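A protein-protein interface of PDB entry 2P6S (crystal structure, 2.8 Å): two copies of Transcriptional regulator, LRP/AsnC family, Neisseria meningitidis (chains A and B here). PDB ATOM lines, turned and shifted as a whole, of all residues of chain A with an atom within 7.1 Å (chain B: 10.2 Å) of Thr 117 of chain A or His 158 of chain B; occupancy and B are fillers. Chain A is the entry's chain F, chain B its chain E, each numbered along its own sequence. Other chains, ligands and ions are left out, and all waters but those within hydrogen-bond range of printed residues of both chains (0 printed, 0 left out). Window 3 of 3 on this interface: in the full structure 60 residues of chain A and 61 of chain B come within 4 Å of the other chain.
Of the printed residues of chain B, Thr 117 of chain A touches His 158 (3.99 Å). Printed residues of chain A within 4 Å of His 158 of chain B: Val 66, Asn 67, Leu 68 and Thr 117. Of chain B, only His 158 (3.8 Å) and Leu 159 (3.6 Å) come within 4 Å of Asn 67 of chain A. Leu 68 of chain A touches three residues of chain B. No residue of chain B comes within 4 Å of Gly 69 of chain A. No residue of chain B comes within 4 Å of Asp 118 of chain A. Of the printed residues of chain B, Pro 63 of chain A touches Leu 154. Of the printed residues of chain A, Leu 154 of chain B touches Pro 63, Val 66, Leu 68 and Phe 115. Of the printed residues of chain B, Phe 115 of chain A touches Leu 154 (3.3 Å). Ile 53 of chain B touches none of the printed residues of chain A. Leu 160 of chain B touches none of the printed residues of chain A. The nearest printed residue of chain B that does not touch Thr 117 of chain A is Pro 155 of chain B (7.4 Å).
Among the printed residues, 12 pairs touch across the chains.
The backbone carbonyl oxygen (O) of Val 66 of chain A sits at hydrogen-bond distance from a ring nitrogen (NE2) of His 158 of chain B (2.6 Å).
The side-chain amide nitrogen of Gln 20 of chain B lies within hydrogen-bond range of the backbone carbonyl oxygen of Leu 154 of chain B, 2.9 Å away. O of Pro 63 of chain A is in hydrogen-bond range of N of Leu 68 of chain A, 2.8 Å away.
No position is printed for both chains. Of the 12 pairs that touch across the chains among the printed residues, none has its exchanged pair printed and touching as well.
Among the printed residues, pairs that only touch across the chains: Pro 63 of chain A with Leu 154 of chain B (3.7 Å), Val 66 of chain A with Leu 154 of chain B (3.996 Å), Val 66 of chain A with Leu 156 of chain B (3.7 Å), Val 66 of chain A with Leu 159 of chain B (3.9 Å), Asn 67 of chain A with His 158 of chain B (3.8 Å), Asn 67 of chain A with Leu 159 of chain B (3.6 Å), Leu 68 of chain A with Leu 154 of chain B (3.8 Å), Leu 68 of chain A with Pro 155 of chain B (3.4 Å), Leu 68 of chain A with His 158 of chain B (3.6 Å), Phe 115 of chain A with Leu 154 of chain B (3.3 Å) and Thr 117 of chain A with His 158 of chain B (3.99 Å).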
ATOM      1  N   PRO A  63       2.411  12.109  29.597  1.00  0.00           N
ATOM      2  CA  PRO A  63       2.758  10.736  29.979  1.00  0.00           C
ATOM      3  C   PRO A  63       2.708  10.439  31.494  1.00  0.00           C
ATOM      4  O   PRO A  63       2.139   9.422  31.899  1.00  0.00           O
ATOM      5  CB  PRO A  63       4.178  10.589  29.432  1.00  0.00           C
ATOM      6  CG  PRO A  63       4.180  11.442  28.207  1.00  0.00           C
ATOM      7  CD  PRO A  63       3.285  12.608  28.517  1.00  0.00           C
ATOM      8  N   VAL A  66      -0.905  10.149  33.052  1.00  0.00           N
ATOM      9  CA  VAL A  66      -1.662   8.915  32.794  1.00  0.00           C
ATOM     10  C   VAL A  66      -0.812   7.660  33.035  1.00  0.00           C
ATOM     11  O   VAL A  66      -0.956   6.657  32.329  1.00  0.00           O
ATOM     12  CB  VAL A  66      -2.236   8.909  31.360  1.00  0.00           C
ATOM     13  CG1 VAL A  66      -3.240  10.032  31.196  1.00  0.00           C
ATOM     14  CG2 VAL A  66      -1.119   9.040  30.321  1.00  0.00           C
ATOM     15  N   ASN A  67       0.068   7.739  34.041  1.00  0.00           N
ATOM     16  CA  ASN A  67       0.900   6.616  34.515  1.00  0.00           C
ATOM     17  C   ASN A  67       2.011   6.149  33.574  1.00  0.00           C
ATOM     18  O   ASN A  67       2.833   5.313  33.969  1.00  0.00           O
ATOM     19  CB  ASN A  67       0.052   5.398  34.915  1.00  0.00           C
ATOM     20  CG  ASN A  67      -0.860   5.676  36.092  1.00  0.00           C
ATOM     21  OD1 ASN A  67      -1.796   6.473  35.999  1.00  0.00           O
ATOM     22  ND2 ASN A  67      -0.605   4.997  37.207  1.00  0.00           N
ATOM     23  N   LEU A  68       2.042   6.680  32.349  1.00  0.00           N
ATOM     24  CA  LEU A  68       3.058   6.302  31.366  1.00  0.00           C
ATOM     25  C   LEU A  68       4.372   6.974  31.733  1.00  0.00           C
ATOM     26  O   LEU A  68       4.645   8.099  31.324  1.00  0.00           O
ATOM     27  CB  LEU A  68       2.616   6.685  29.954  1.00  0.00           C
ATOM     28  CG  LEU A  68       1.410   5.893  29.451  1.00  0.00           C
ATOM     29  CD1 LEU A  68       0.856   6.497  28.168  1.00  0.00           C
ATOM     30  CD2 LEU A  68       1.777   4.422  29.252  1.00  0.00           C
ATOM     31  N   GLY A  69       5.176   6.273  32.527  1.00  0.00           N
ATOM     32  CA  GLY A  69       6.401   6.841  33.092  1.00  0.00           C
ATOM     33  C   GLY A  69       7.664   6.423  32.369  1.00  0.00           C
ATOM     34  O   GLY A  69       8.768   6.858  32.737  1.00  0.00           O
ATOM     35  N   LEU A  70       7.503   5.586  31.340  1.00  0.00           N
ATOM     36  CA  LEU A  70       8.641   5.015  30.631  1.00  0.00           C
ATOM     37  C   LEU A  70       8.492   5.237  29.129  1.00  0.00           C
ATOM     38  O   LEU A  70       7.672   4.589  28.470  1.00  0.00           O
ATOM     39  CB  LEU A  70       8.775   3.522  30.970  1.00  0.00           C
ATOM     40  CG  LEU A  70      10.051   2.758  30.595  1.00  0.00           C
ATOM     41  CD1 LEU A  70      11.294   3.537  30.918  1.00  0.00           C
ATOM     42  CD2 LEU A  70      10.083   1.424  31.312  1.00  0.00           C
ATOM     43  N   PHE A 115       5.607   3.982  24.555  1.00  0.00           N
ATOM     44  CA  PHE A 115       5.244   4.447  25.892  1.00  0.00           C
ATOM     45  C   PHE A 115       4.710   3.339  26.776  1.00  0.00           C
ATOM     46  O   PHE A 115       3.815   2.602  26.377  1.00  0.00           O
ATOM     47  CB  PHE A 115       4.199   5.546  25.791  1.00  0.00           C
ATOM     48  CG  PHE A 115       4.786   6.916  25.700  1.00  0.00           C
ATOM     49  CD1 PHE A 115       5.225   7.568  26.843  1.00  0.00           C
ATOM     50  CD2 PHE A 115       4.917   7.551  24.481  1.00  0.00           C
ATOM     51  CE1 PHE A 115       5.777   8.831  26.771  1.00  0.00           C
ATOM     52  CE2 PHE A 115       5.467   8.815  24.405  1.00  0.00           C
ATOM     53  CZ  PHE A 115       5.900   9.453  25.553  1.00  0.00           C
ATOM     54  N   PHE A 116       5.247   3.234  27.985  1.00  0.00           N
ATOM     55  CA  PHE A 116       4.887   2.151  28.893  1.00  0.00           C
ATOM     56  C   PHE A 116       4.713   2.660  30.314  1.00  0.00           C
ATOM     57  O   PHE A 116       5.275   3.697  30.692  1.00  0.00           O
ATOM     58  CB  PHE A 116       5.963   1.065  28.856  1.00  0.00           C
ATOM     59  CG  PHE A 116       6.201   0.507  27.485  1.00  0.00           C
ATOM     60  CD1 PHE A 116       5.431  -0.541  27.006  1.00  0.00           C
ATOM     61  CD2 PHE A 116       7.172   1.054  26.658  1.00  0.00           C
ATOM     62  CE1 PHE A 116       5.640  -1.050  25.730  1.00  0.00           C
ATOM     63  CE2 PHE A 116       7.384   0.553  25.381  1.00  0.00           C
ATOM     64  CZ  PHE A 116       6.621  -0.503  24.917  1.00  0.00           C
ATOM     65  N   THR A 117       3.929   1.927  31.100  1.00  0.00           N
ATOM     66  CA  THR A 117       3.691   2.303  32.489  1.00  0.00           C
ATOM     67  C   THR A 117       4.974   2.157  33.293  1.00  0.00           C
ATOM     68  O   THR A 117       5.315   3.047  34.067  1.00  0.00           O
ATOM     69  CB  THR A 117       2.521   1.510  33.167  1.00  0.00           C
ATOM     70  OG1 THR A 117       2.952   1.012  34.441  1.00  0.00           O
ATOM     71  CG2 THR A 117       2.032   0.333  32.312  1.00  0.00           C
ATOM     72  N   ASP A 118       5.682   1.044  33.100  1.00  0.00           N
ATOM     73  CA  ASP A 118       6.935   0.767  33.820  1.00  0.00           C
ATOM     74  C   ASP A 118       7.780  -0.280  33.078  1.00  0.00           C
ATOM     75  O   ASP A 118       7.397  -0.716  31.990  1.00  0.00           O
ATOM     76  CB  ASP A 118       6.628   0.312  35.256  1.00  0.00           C
ATOM     77  CG  ASP A 118       5.848  -0.996  35.313  1.00  0.00           C
ATOM     78  OD1 ASP A 118       5.821  -1.733  34.303  1.00  0.00           O
ATOM     79  OD2 ASP A 118       5.271  -1.290  36.381  1.00  0.00           O
ATOM     80  N   MET A 119       8.914  -0.682  33.663  1.00  0.00           N
ATOM     81  CA  MET A 119       9.811  -1.663  33.033  1.00  0.00           C
ATOM     82  C   MET A 119       9.191  -3.065  32.895  1.00  0.00           C
ATOM     83  O   MET A 119       9.483  -3.773  31.923  1.00  0.00           O
ATOM     84  CB  MET A 119      11.137  -1.764  33.788  1.00  0.00           C
ATOM     85  CG  MET A 119      12.225  -2.542  33.032  1.00  0.00           C
ATOM     86  SD  MET A 119      12.820  -1.681  31.366  1.00  0.00           S
ATOM     87  CE  MET A 119      14.047  -0.379  32.134  1.00  0.00           C
ATOM     88  N   ASN A 120       8.356  -3.469  33.858  1.00  0.00           N
ATOM     89  CA  ASN A 120       7.632  -4.736  33.743  1.00  0.00           C
ATOM     90  C   ASN A 120       6.744  -4.742  32.514  1.00  0.00           C
ATOM     91  O   ASN A 120       6.711  -5.723  31.775  1.00  0.00           O
ATOM     92  CB  ASN A 120       6.784  -5.023  34.985  1.00  0.00           C
ATOM     93  CG  ASN A 120       7.617  -5.461  36.179  1.00  0.00           C
ATOM     94  OD1 ASN A 120       8.493  -6.324  36.064  1.00  0.00           O
ATOM     95  ND2 ASN A 120       7.342  -4.868  37.337  1.00  0.00           N
ATOM     96  N   ALA A 121       6.031  -3.637  32.299  1.00  0.00           N
ATOM     97  CA  ALA A 121       5.200  -3.468  31.107  1.00  0.00           C
ATOM     98  C   ALA A 121       6.056  -3.582  29.859  1.00  0.00           C
ATOM     99  O   ALA A 121       5.693  -4.276  28.908  1.00  0.00           O
ATOM    100  CB  ALA A 121       4.484  -2.122  31.126  1.00  0.00           C
ATOM    101  N   PHE A 122       7.201  -2.914  29.874  1.00  0.00           N
ATOM    102  CA  PHE A 122       8.109  -2.963  28.741  1.00  0.00           C
ATOM    103  C   PHE A 122       8.568  -4.384  28.459  1.00  0.00           C
ATOM    104  O   PHE A 122       8.520  -4.845  27.326  1.00  0.00           O
ATOM    105  CB  PHE A 122       9.334  -2.093  28.992  1.00  0.00           C
ATOM    106  CG  PHE A 122      10.173  -1.883  27.771  1.00  0.00           C
ATOM    107  CD1 PHE A 122       9.797  -0.948  26.831  1.00  0.00           C
ATOM    108  CD2 PHE A 122      11.333  -2.620  27.558  1.00  0.00           C
ATOM    109  CE1 PHE A 122      10.555  -0.739  25.694  1.00  0.00           C
ATOM    110  CE2 PHE A 122      12.101  -2.419  26.429  1.00  0.00           C
ATOM    111  CZ  PHE A 122      11.711  -1.477  25.491  1.00  0.00           C
ATOM    112  N   LEU B   8      -9.708   9.433  37.721  1.00  0.00           N
ATOM    113  CA  LEU B   8     -10.375   9.332  36.408  1.00  0.00           C
ATOM    114  C   LEU B   8     -11.463   8.261  36.354  1.00  0.00           C
ATOM    115  O   LEU B   8     -11.436   7.293  37.109  1.00  0.00           O
ATOM    116  CB  LEU B   8      -9.350   9.047  35.304  1.00  0.00           C
ATOM    117  CG  LEU B   8      -8.313  10.142  35.041  1.00  0.00           C
ATOM    118  CD1 LEU B   8      -7.329   9.701  33.975  1.00  0.00           C
ATOM    119  CD2 LEU B   8      -8.990  11.441  34.633  1.00  0.00           C
ATOM    120  N   ILE B  13     -11.741   8.902  30.381  1.00  0.00           N
ATOM    121  CA  ILE B  13     -10.784   8.305  29.456  1.00  0.00           C
ATOM    122  C   ILE B  13     -11.257   8.439  28.004  1.00  0.00           C
ATOM    123  O   ILE B  13     -10.479   8.832  27.132  1.00  0.00           O
ATOM    124  CB  ILE B  13     -10.528   6.812  29.781  1.00  0.00           C
ATOM    125  CG1 ILE B  13      -9.914   6.656  31.177  1.00  0.00           C
ATOM    126  CG2 ILE B  13      -9.617   6.180  28.737  1.00  0.00           C
ATOM    127  CD1 ILE B  13      -8.757   7.601  31.470  1.00  0.00           C
ATOM    128  N   LEU B  16     -10.538  11.951  26.604  1.00  0.00           N
ATOM    129  CA  LEU B  16      -9.142  12.101  26.199  1.00  0.00           C
ATOM    130  C   LEU B  16      -8.929  11.397  24.867  1.00  0.00           C
ATOM    131  O   LEU B  16      -8.431  11.987  23.908  1.00  0.00           O
ATOM    132  CB  LEU B  16      -8.220  11.479  27.232  1.00  0.00           C
ATOM    133  CG  LEU B  16      -8.204  12.135  28.599  1.00  0.00           C
ATOM    134  CD1 LEU B  16      -7.630  11.175  29.639  1.00  0.00           C
ATOM    135  CD2 LEU B  16      -7.412  13.427  28.515  1.00  0.00           C
ATOM    136  N   GLN B  17      -9.343  10.131  24.821  1.00  0.00           N
ATOM    137  CA  GLN B  17      -9.195   9.274  23.639  1.00  0.00           C
ATOM    138  C   GLN B  17      -9.836   9.868  22.380  1.00  0.00           C
ATOM    139  O   GLN B  17      -9.343   9.665  21.272  1.00  0.00           O
ATOM    140  CB  GLN B  17      -9.782   7.888  23.932  1.00  0.00           C
ATOM    141  CG  GLN B  17      -8.953   7.090  24.946  1.00  0.00           C
ATOM    142  CD  GLN B  17      -9.582   5.765  25.329  1.00  0.00           C
ATOM    143  OE1 GLN B  17     -10.799   5.582  25.234  1.00  0.00           O
ATOM    144  NE2 GLN B  17      -8.747   4.828  25.772  1.00  0.00           N
ATOM    145  N   GLN B  20      -7.574  13.460  21.718  1.00  0.00           N
ATOM    146  CA  GLN B  20      -6.233  13.221  21.182  1.00  0.00           C
ATOM    147  C   GLN B  20      -6.251  13.120  19.654  1.00  0.00           C
ATOM    148  O   GLN B  20      -5.316  13.578  18.995  1.00  0.00           O
ATOM    149  CB  GLN B  20      -5.622  11.944  21.781  1.00  0.00           C
ATOM    150  CG  GLN B  20      -5.206  12.065  23.239  1.00  0.00           C
ATOM    151  CD  GLN B  20      -4.175  11.025  23.662  1.00  0.00           C
ATOM    152  OE1 GLN B  20      -3.094  11.370  24.141  1.00  0.00           O
ATOM    153  NE2 GLN B  20      -4.506   9.749  23.494  1.00  0.00           N
ATOM    154  N   ILE B  53      -3.416  17.038  32.865  1.00  0.00           N
ATOM    155  CA  ILE B  53      -3.523  15.872  31.975  1.00  0.00           C
ATOM    156  C   ILE B  53      -3.333  16.335  30.531  1.00  0.00           C
ATOM    157  O   ILE B  53      -2.412  15.890  29.852  1.00  0.00           O
ATOM    158  CB  ILE B  53      -4.893  15.121  32.124  1.00  0.00           C
ATOM    159  CG1 ILE B  53      -5.011  14.383  33.464  1.00  0.00           C
ATOM    160  CG2 ILE B  53      -5.083  14.101  31.009  1.00  0.00           C
ATOM    161  CD1 ILE B  53      -4.247  15.001  34.613  1.00  0.00           C
ATOM    162  N   LEU B 154      -1.289   9.025  23.007  1.00  0.00           N
ATOM    163  CA  LEU B 154      -0.820   8.062  24.002  1.00  0.00           C
ATOM    164  C   LEU B 154      -1.888   7.007  24.237  1.00  0.00           C
ATOM    165  O   LEU B 154      -3.076   7.307  24.118  1.00  0.00           O
ATOM    166  CB  LEU B 154      -0.539   8.751  25.341  1.00  0.00           C
ATOM    167  CG  LEU B 154       0.686   9.641  25.516  1.00  0.00           C
ATOM    168  CD1 LEU B 154       0.764  10.100  26.960  1.00  0.00           C
ATOM    169  CD2 LEU B 154       1.955   8.905  25.120  1.00  0.00           C
ATOM    170  N   PRO B 155      -1.475   5.774  24.597  1.00  0.00           N
ATOM    171  CA  PRO B 155      -2.424   4.724  24.981  1.00  0.00           C
ATOM    172  C   PRO B 155      -2.965   4.954  26.385  1.00  0.00           C
ATOM    173  O   PRO B 155      -2.210   5.358  27.273  1.00  0.00           O
ATOM    174  CB  PRO B 155      -1.573   3.459  24.954  1.00  0.00           C
ATOM    175  CG  PRO B 155      -0.205   3.940  25.308  1.00  0.00           C
ATOM    176  CD  PRO B 155      -0.080   5.296  24.663  1.00  0.00           C
ATOM    177  N   LEU B 156      -4.258   4.698  26.577  1.00  0.00           N
ATOM    178  CA  LEU B 156      -4.927   4.939  27.857  1.00  0.00           C
ATOM    179  C   LEU B 156      -5.741   3.736  28.345  1.00  0.00           C
ATOM    180  O   LEU B 156      -6.507   3.852  29.302  1.00  0.00           O
ATOM    181  CB  LEU B 156      -5.839   6.164  27.731  1.00  0.00           C
ATOM    182  CG  LEU B 156      -5.183   7.458  27.227  1.00  0.00           C
ATOM    183  CD1 LEU B 156      -6.232   8.523  26.943  1.00  0.00           C
ATOM    184  CD2 LEU B 156      -4.133   7.979  28.215  1.00  0.00           C
ATOM    185  N   ASN B 157      -5.566   2.582  27.700  1.00  0.00           N
ATOM    186  CA  ASN B 157      -6.310   1.367  28.060  1.00  0.00           C
ATOM    187  C   ASN B 157      -5.788   0.714  29.329  1.00  0.00           C
ATOM    188  O   ASN B 157      -6.451  -0.145  29.907  1.00  0.00           O
ATOM    189  CB  ASN B 157      -6.281   0.351  26.914  1.00  0.00           C
ATOM    190  CG  ASN B 157      -7.081   0.813  25.706  1.00  0.00           C
ATOM    191  OD1 ASN B 157      -6.566   0.860  24.586  1.00  0.00           O
ATOM    192  ND2 ASN B 157      -8.347   1.165  25.930  1.00  0.00           N
ATOM    193  N   HIS B 158      -4.596   1.125  29.752  1.00  0.00           N
ATOM    194  CA  HIS B 158      -4.025   0.674  31.012  1.00  0.00           C
ATOM    195  C   HIS B 158      -4.677   1.333  32.234  1.00  0.00           C
ATOM    196  O   HIS B 158      -4.399   0.931  33.359  1.00  0.00           O
ATOM    197  CB  HIS B 158      -2.507   0.893  31.014  1.00  0.00           C
ATOM    198  CG  HIS B 158      -2.096   2.325  31.139  1.00  0.00           C
ATOM    199  ND1 HIS B 158      -2.912   3.371  30.771  1.00  0.00           N
ATOM    200  CD2 HIS B 158      -0.941   2.885  31.571  1.00  0.00           C
ATOM    201  CE1 HIS B 158      -2.286   4.514  30.984  1.00  0.00           C
ATOM    202  NE2 HIS B 158      -1.088   4.248  31.471  1.00  0.00           N
ATOM    203  N   LEU B 159      -5.537   2.330  32.018  1.00  0.00           N
ATOM    204  CA  LEU B 159      -6.277   2.973  33.115  1.00  0.00           C
ATOM    205  C   LEU B 159      -7.639   2.341  33.403  1.00  0.00           C
ATOM    206  O   LEU B 159      -8.261   2.676  34.406  1.00  0.00           O
ATOM    207  CB  LEU B 159      -6.483   4.459  32.828  1.00  0.00           C
ATOM    208  CG  LEU B 159      -5.214   5.255  32.533  1.00  0.00           C
ATOM    209  CD1 LEU B 159      -5.554   6.682  32.141  1.00  0.00           C
ATOM    210  CD2 LEU B 159      -4.265   5.228  33.721  1.00  0.00           C
ATOM    211  N   LEU B 160      -8.100   1.439  32.537  1.00  0.00           N
ATOM    212  CA  LEU B 160      -9.421   0.799  32.698  1.00  0.00           C
ATOM    213  C   LEU B 160      -9.360  -0.580  33.377  1.00  0.00           C
ATOM    214  O   LEU B 160      -8.297  -1.179  33.554  1.00  0.00           O
ATOM    215  CB  LEU B 160     -10.117   0.680  31.338  1.00  0.00           C
ATOM    216  CG  LEU B 160     -10.591   2.009  30.749  1.00  0.00           C
ATOM    217  CD1 LEU B 160     -10.922   1.860  29.270  1.00  0.00           C
ATOM    218  CD2 LEU B 160     -11.782   2.525  31.536  1.00  0.00           C
